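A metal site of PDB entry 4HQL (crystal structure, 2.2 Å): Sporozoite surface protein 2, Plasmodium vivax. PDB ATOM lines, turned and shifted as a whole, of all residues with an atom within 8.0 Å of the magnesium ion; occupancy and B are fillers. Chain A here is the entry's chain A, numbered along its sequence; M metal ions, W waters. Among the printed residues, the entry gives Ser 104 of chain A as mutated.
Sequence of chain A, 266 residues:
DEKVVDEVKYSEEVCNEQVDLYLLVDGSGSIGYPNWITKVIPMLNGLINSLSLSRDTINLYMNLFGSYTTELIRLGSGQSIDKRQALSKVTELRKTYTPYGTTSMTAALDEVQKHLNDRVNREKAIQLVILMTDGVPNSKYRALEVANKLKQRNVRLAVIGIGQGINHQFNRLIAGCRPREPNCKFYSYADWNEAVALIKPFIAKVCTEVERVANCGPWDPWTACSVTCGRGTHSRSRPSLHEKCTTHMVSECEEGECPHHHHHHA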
ATOM      1  N   ASP A  26      -5.107  -1.115  12.399  1.00  0.00           N
ATOM      2  CA  ASP A  26      -5.085  -1.165  13.857  1.00  0.00           C
ATOM      3  C   ASP A  26      -3.972  -2.118  14.348  1.00  0.00           C
ATOM      4  O   ASP A  26      -4.065  -3.329  14.178  1.00  0.00           O
ATOM      5  CB  ASP A  26      -6.438  -1.674  14.345  1.00  0.00           C
ATOM      6  CG  ASP A  26      -6.652  -1.489  15.837  1.00  0.00           C
ATOM      7  OD1 ASP A  26      -5.665  -1.473  16.609  1.00  0.00           O
ATOM      8  OD2 ASP A  26      -7.832  -1.372  16.241  1.00  0.00           O
ATOM      9  N   GLY A  27      -2.921  -1.567  14.941  1.00  0.00           N
ATOM     10  CA  GLY A  27      -1.857  -2.397  15.507  1.00  0.00           C
ATOM     11  C   GLY A  27      -1.833  -2.334  17.026  1.00  0.00           C
ATOM     12  O   GLY A  27      -0.788  -2.522  17.660  1.00  0.00           O
ATOM     13  N   SER A  28      -2.996  -2.068  17.630  1.00  0.00           N
ATOM     14  CA  SER A  28      -3.096  -1.829  19.076  1.00  0.00           C
ATOM     15  C   SER A  28      -3.161  -3.135  19.863  1.00  0.00           C
ATOM     16  O   SER A  28      -3.387  -4.221  19.296  1.00  0.00           O
ATOM     17  CB  SER A  28      -4.332  -0.984  19.376  1.00  0.00           C
ATOM     18  OG  SER A  28      -5.524  -1.727  19.195  1.00  0.00           O
ATOM     19  N   GLY A  29      -2.966  -3.041  21.179  1.00  0.00           N
ATOM     20  CA  GLY A  29      -2.882  -4.237  22.031  1.00  0.00           C
ATOM     21  C   GLY A  29      -4.149  -5.064  22.101  1.00  0.00           C
ATOM     22  O   GLY A  29      -4.091  -6.249  22.373  1.00  0.00           O
ATOM     23  N   SER A  30      -5.304  -4.453  21.847  1.00  0.00           N
ATOM     24  CA  SER A  30      -6.561  -5.209  21.816  1.00  0.00           C
ATOM     25  C   SER A  30      -6.639  -6.230  20.650  1.00  0.00           C
ATOM     26  O   SER A  30      -7.432  -7.161  20.685  1.00  0.00           O
ATOM     27  CB  SER A  30      -7.779  -4.259  21.752  1.00  0.00           C
ATOM     28  OG  SER A  30      -7.706  -3.399  20.617  1.00  0.00           O
ATOM     29  N   ILE A  31      -5.835  -6.048  19.609  1.00  0.00           N
ATOM     30  CA  ILE A  31      -5.923  -6.947  18.433  1.00  0.00           C
ATOM     31  C   ILE A  31      -5.668  -8.405  18.842  1.00  0.00           C
ATOM     32  O   ILE A  31      -6.460  -9.298  18.522  1.00  0.00           O
ATOM     33  CB  ILE A  31      -4.992  -6.517  17.269  1.00  0.00           C
ATOM     34  CG1 ILE A  31      -5.470  -5.184  16.670  1.00  0.00           C
ATOM     35  CG2 ILE A  31      -4.891  -7.626  16.194  1.00  0.00           C
ATOM     36  CD1 ILE A  31      -6.981  -5.094  16.409  1.00  0.00           C
ATOM     37  N   GLY A  32      -4.593  -8.632  19.597  1.00  0.00           N
ATOM     38  CA  GLY A  32      -4.270  -9.971  20.051  1.00  0.00           C
ATOM     39  C   GLY A  32      -3.177 -10.521  19.137  1.00  0.00           C
ATOM     40  O   GLY A  32      -3.301 -10.443  17.914  1.00  0.00           O
ATOM     41  N   PHE A  65      -1.666   2.183  13.312  1.00  0.00           N
ATOM     42  CA  PHE A  65      -2.019   2.969  14.494  1.00  0.00           C
ATOM     43  C   PHE A  65      -2.143   2.138  15.757  1.00  0.00           C
ATOM     44  O   PHE A  65      -2.812   1.112  15.778  1.00  0.00           O
ATOM     45  CB  PHE A  65      -3.248   3.867  14.290  1.00  0.00           C
ATOM     46  CG  PHE A  65      -4.542   3.122  14.012  1.00  0.00           C
ATOM     47  CD1 PHE A  65      -4.893   2.759  12.713  1.00  0.00           C
ATOM     48  CD2 PHE A  65      -5.430   2.855  15.057  1.00  0.00           C
ATOM     49  CE1 PHE A  65      -6.100   2.112  12.466  1.00  0.00           C
ATOM     50  CE2 PHE A  65      -6.656   2.198  14.817  1.00  0.00           C
ATOM     51  CZ  PHE A  65      -6.983   1.840  13.518  1.00  0.00           C
ATOM     52  N   GLY A  66      -1.436   2.586  16.785  1.00  0.00           N
ATOM     53  CA  GLY A  66      -1.426   1.962  18.089  1.00  0.00           C
ATOM     54  C   GLY A  66      -1.416   3.113  19.083  1.00  0.00           C
ATOM     55  O   GLY A  66      -2.264   4.005  18.992  1.00  0.00           O
ATOM     56  N   TYR A 100       0.449  -3.758  20.377  1.00  0.00           N
ATOM     57  CA  TYR A 100       0.526  -3.331  21.765  1.00  0.00           C
ATOM     58  C   TYR A 100      -0.070  -1.932  21.860  1.00  0.00           C
ATOM     59  O   TYR A 100      -0.192  -1.227  20.860  1.00  0.00           O
ATOM     60  CB  TYR A 100       1.990  -3.307  22.264  1.00  0.00           C
ATOM     61  CG  TYR A 100       2.705  -2.034  21.868  1.00  0.00           C
ATOM     62  CD1 TYR A 100       3.247  -1.886  20.586  1.00  0.00           C
ATOM     63  CD2 TYR A 100       2.814  -0.945  22.749  1.00  0.00           C
ATOM     64  CE1 TYR A 100       3.900  -0.707  20.187  1.00  0.00           C
ATOM     65  CE2 TYR A 100       3.459   0.257  22.356  1.00  0.00           C
ATOM     66  CZ  TYR A 100       3.993   0.356  21.076  1.00  0.00           C
ATOM     67  OH  TYR A 100       4.636   1.516  20.656  1.00  0.00           O
ATOM     68  N   GLY A 101      -0.417  -1.531  23.073  1.00  0.00           N
ATOM     69  CA  GLY A 101      -0.720  -0.147  23.353  1.00  0.00           C
ATOM     70  C   GLY A 101      -2.166   0.260  23.104  1.00  0.00           C
ATOM     71  O   GLY A 101      -3.058  -0.571  22.897  1.00  0.00           O
ATOM     72  N   THR A 102      -2.387   1.564  23.115  1.00  0.00           N
ATOM     73  CA  THR A 102      -3.719   2.097  22.881  1.00  0.00           C
ATOM     74  C   THR A 102      -4.009   2.187  21.378  1.00  0.00           C
ATOM     75  O   THR A 102      -3.291   1.591  20.565  1.00  0.00           O
ATOM     76  CB  THR A 102      -3.932   3.444  23.648  1.00  0.00           C
ATOM     77  OG1 THR A 102      -2.834   4.330  23.389  1.00  0.00           O
ATOM     78  CG2 THR A 102      -3.974   3.179  25.178  1.00  0.00           C
ATOM     79  N   THR A 103      -5.061   2.901  21.005  1.00  0.00           N
ATOM     80  CA  THR A 103      -5.632   2.769  19.684  1.00  0.00           C
ATOM     81  C   THR A 103      -5.915   4.147  19.072  1.00  0.00           C
ATOM     82  O   THR A 103      -7.025   4.676  19.194  1.00  0.00           O
ATOM     83  CB  THR A 103      -6.931   1.960  19.733  1.00  0.00           C
ATOM     84  OG1 THR A 103      -6.729   0.783  20.511  1.00  0.00           O
ATOM     85  CG2 THR A 103      -7.403   1.556  18.296  1.00  0.00           C
ATOM     86  N   SER A 104      -4.915   4.731  18.412  1.00  0.00           N
ATOM     87  CA  SER A 104      -5.024   6.126  17.952  1.00  0.00           C
ATOM     88  C   SER A 104      -5.771   6.197  16.629  1.00  0.00           C
ATOM     89  O   SER A 104      -5.187   6.570  15.609  1.00  0.00           O
ATOM     90  CB  SER A 104      -3.640   6.748  17.786  1.00  0.00           C
ATOM     91  OG  SER A 104      -2.997   6.832  19.037  1.00  0.00           O
ATOM     92  N   MET A 105      -7.044   5.827  16.658  1.00  0.00           N
ATOM     93  CA  MET A 105      -7.814   5.685  15.433  1.00  0.00           C
ATOM     94  C   MET A 105      -8.126   7.065  14.843  1.00  0.00           C
ATOM     95  O   MET A 105      -7.968   7.288  13.652  1.00  0.00           O
ATOM     96  CB  MET A 105      -9.100   4.901  15.687  1.00  0.00           C
ATOM     97  CG  MET A 105      -9.918   4.651  14.423  1.00  0.00           C
ATOM     98  SD  MET A 105     -11.546   3.984  14.765  1.00  0.00           S
ATOM     99  CE  MET A 105     -11.057   2.360  15.372  1.00  0.00           C
ATOM    100  N   THR A 133      -9.862  -2.594  11.654  1.00  0.00           N
ATOM    101  CA  THR A 133      -9.867  -2.380  13.099  1.00  0.00           C
ATOM    102  C   THR A 133     -10.813  -3.321  13.859  1.00  0.00           C
ATOM    103  O   THR A 133     -11.717  -3.905  13.264  1.00  0.00           O
ATOM    104  CB  THR A 133     -10.221  -0.886  13.420  1.00  0.00           C
ATOM    105  OG1 THR A 133     -10.197  -0.673  14.828  1.00  0.00           O
ATOM    106  CG2 THR A 133     -11.621  -0.525  12.880  1.00  0.00           C
ATOM    107  N   ASP A 134     -10.605  -3.464  15.175  1.00  0.00           N
ATOM    108  CA  ASP A 134     -11.585  -4.157  15.999  1.00  0.00           C
ATOM    109  C   ASP A 134     -12.689  -3.209  16.485  1.00  0.00           C
ATOM    110  O   ASP A 134     -13.649  -3.621  17.146  1.00  0.00           O
ATOM    111  CB  ASP A 134     -10.923  -4.898  17.187  1.00  0.00           C
ATOM    112  CG  ASP A 134     -10.239  -3.950  18.187  1.00  0.00           C
ATOM    113  OD1 ASP A 134     -10.396  -2.713  18.121  1.00  0.00           O
ATOM    114  OD2 ASP A 134      -9.529  -4.484  19.071  1.00  0.00           O
ATOM    115  N   GLY A 135     -12.553  -1.938  16.143  1.00  0.00           N
ATOM    116  CA  GLY A 135     -13.606  -0.980  16.415  1.00  0.00           C
ATOM    117  C   GLY A 135     -13.673  -0.507  17.854  1.00  0.00           C
ATOM    118  O   GLY A 135     -14.728  -0.142  18.348  1.00  0.00           O
ATOM    119  N   VAL A 136     -12.523  -0.487  18.523  1.00  0.00           N
ATOM    120  CA  VAL A 136     -12.443  -0.036  19.910  1.00  0.00           C
ATOM    121  C   VAL A 136     -11.375   1.053  20.021  1.00  0.00           C
ATOM    122  O   VAL A 136     -10.262   0.802  20.464  1.00  0.00           O
ATOM    123  CB  VAL A 136     -12.140  -1.191  20.883  1.00  0.00           C
ATOM    124  CG1 VAL A 136     -12.202  -0.692  22.364  1.00  0.00           C
ATOM    125  CG2 VAL A 136     -13.133  -2.315  20.680  1.00  0.00           C
ATOM    126  N   PRO A 137     -11.714   2.285  19.619  1.00  0.00           N
ATOM    127  CA  PRO A 137     -10.744   3.375  19.520  1.00  0.00           C
ATOM    128  C   PRO A 137     -10.479   3.982  20.891  1.00  0.00           C
ATOM    129  O   PRO A 137     -11.228   3.684  21.842  1.00  0.00           O
ATOM    130  CB  PRO A 137     -11.475   4.380  18.616  1.00  0.00           C
ATOM    131  CG  PRO A 137     -12.909   4.230  19.039  1.00  0.00           C
ATOM    132  CD  PRO A 137     -13.075   2.728  19.247  1.00  0.00           C
ATOM    133  N   ASN A 138      -9.459   4.822  21.010  1.00  0.00           N
ATOM    134  CA  ASN A 138      -9.262   5.560  22.252  1.00  0.00           C
ATOM    135  C   ASN A 138     -10.507   6.376  22.652  1.00  0.00           C
ATOM    136  O   ASN A 138     -10.776   6.544  23.835  1.00  0.00           O
ATOM    137  CB  ASN A 138      -8.045   6.478  22.195  1.00  0.00           C
ATOM    138  CG  ASN A 138      -6.724   5.701  22.131  1.00  0.00           C
ATOM    139  OD1 ASN A 138      -6.657   4.525  22.487  1.00  0.00           O
ATOM    140  ND2 ASN A 138      -5.674   6.387  21.702  1.00  0.00           N
ATOM    141  N   GLY A 165     -11.472  -9.468  19.509  1.00  0.00           N
ATOM    142  CA  GLY A 165     -12.720  -9.006  20.110  1.00  0.00           C
ATOM    143  C   GLY A 165     -13.291  -7.829  19.347  1.00  0.00           C
ATOM    144  O   GLY A 165     -13.074  -6.673  19.714  1.00  0.00           O
HETATM  145 MG    MG M   1      -7.180  -1.352  20.430  1.00  0.00          MG
HETATM  146  O   HOH W   1      -5.981  -1.588  22.059  1.00  0.00           O
HETATM  147  O   HOH W   2      -8.430  -1.378  18.716  1.00  0.00           O
HETATM  148  O   HOH W   3      -8.755  -0.884  21.709  1.00  0.00           O
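The magnesium ion is bound by water W1, water W3, the side-chain hydroxyl of Ser 28, water W2, the side-chain hydroxyl of Ser 30 and the side-chain hydroxyl of Thr 103. The magnesium ion has six donor atoms within binding distance.
Val 136 touches the magnesium ion (O to MG, 3.8 Å). The nearest printed residue that does not touch the magnesium ion is Asp 26 (4.1 Å).
Water W1 lies within hydrogen-bond range of N of Ser 30 (3.0 Å), O of Gly 101 (3.2 Å) and N of Gly 29 (3.5 Å).
The backbone NH of Ser 28 lies within hydrogen-bond range of the side-chain carboxylate of Asp 26, at 2.9 Å. The side-chain carboxylate of Asp 134 lies close to the side-chain hydroxyl of Ser 30. The side-chain amide oxygen of Asn 138 sits at hydrogen-bond distance from the backbone NH of Thr 103, 2.7 Å away. OD1 of Asp 134 lies within hydrogen-bond range of N of Val 136, 3.1 Å away.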
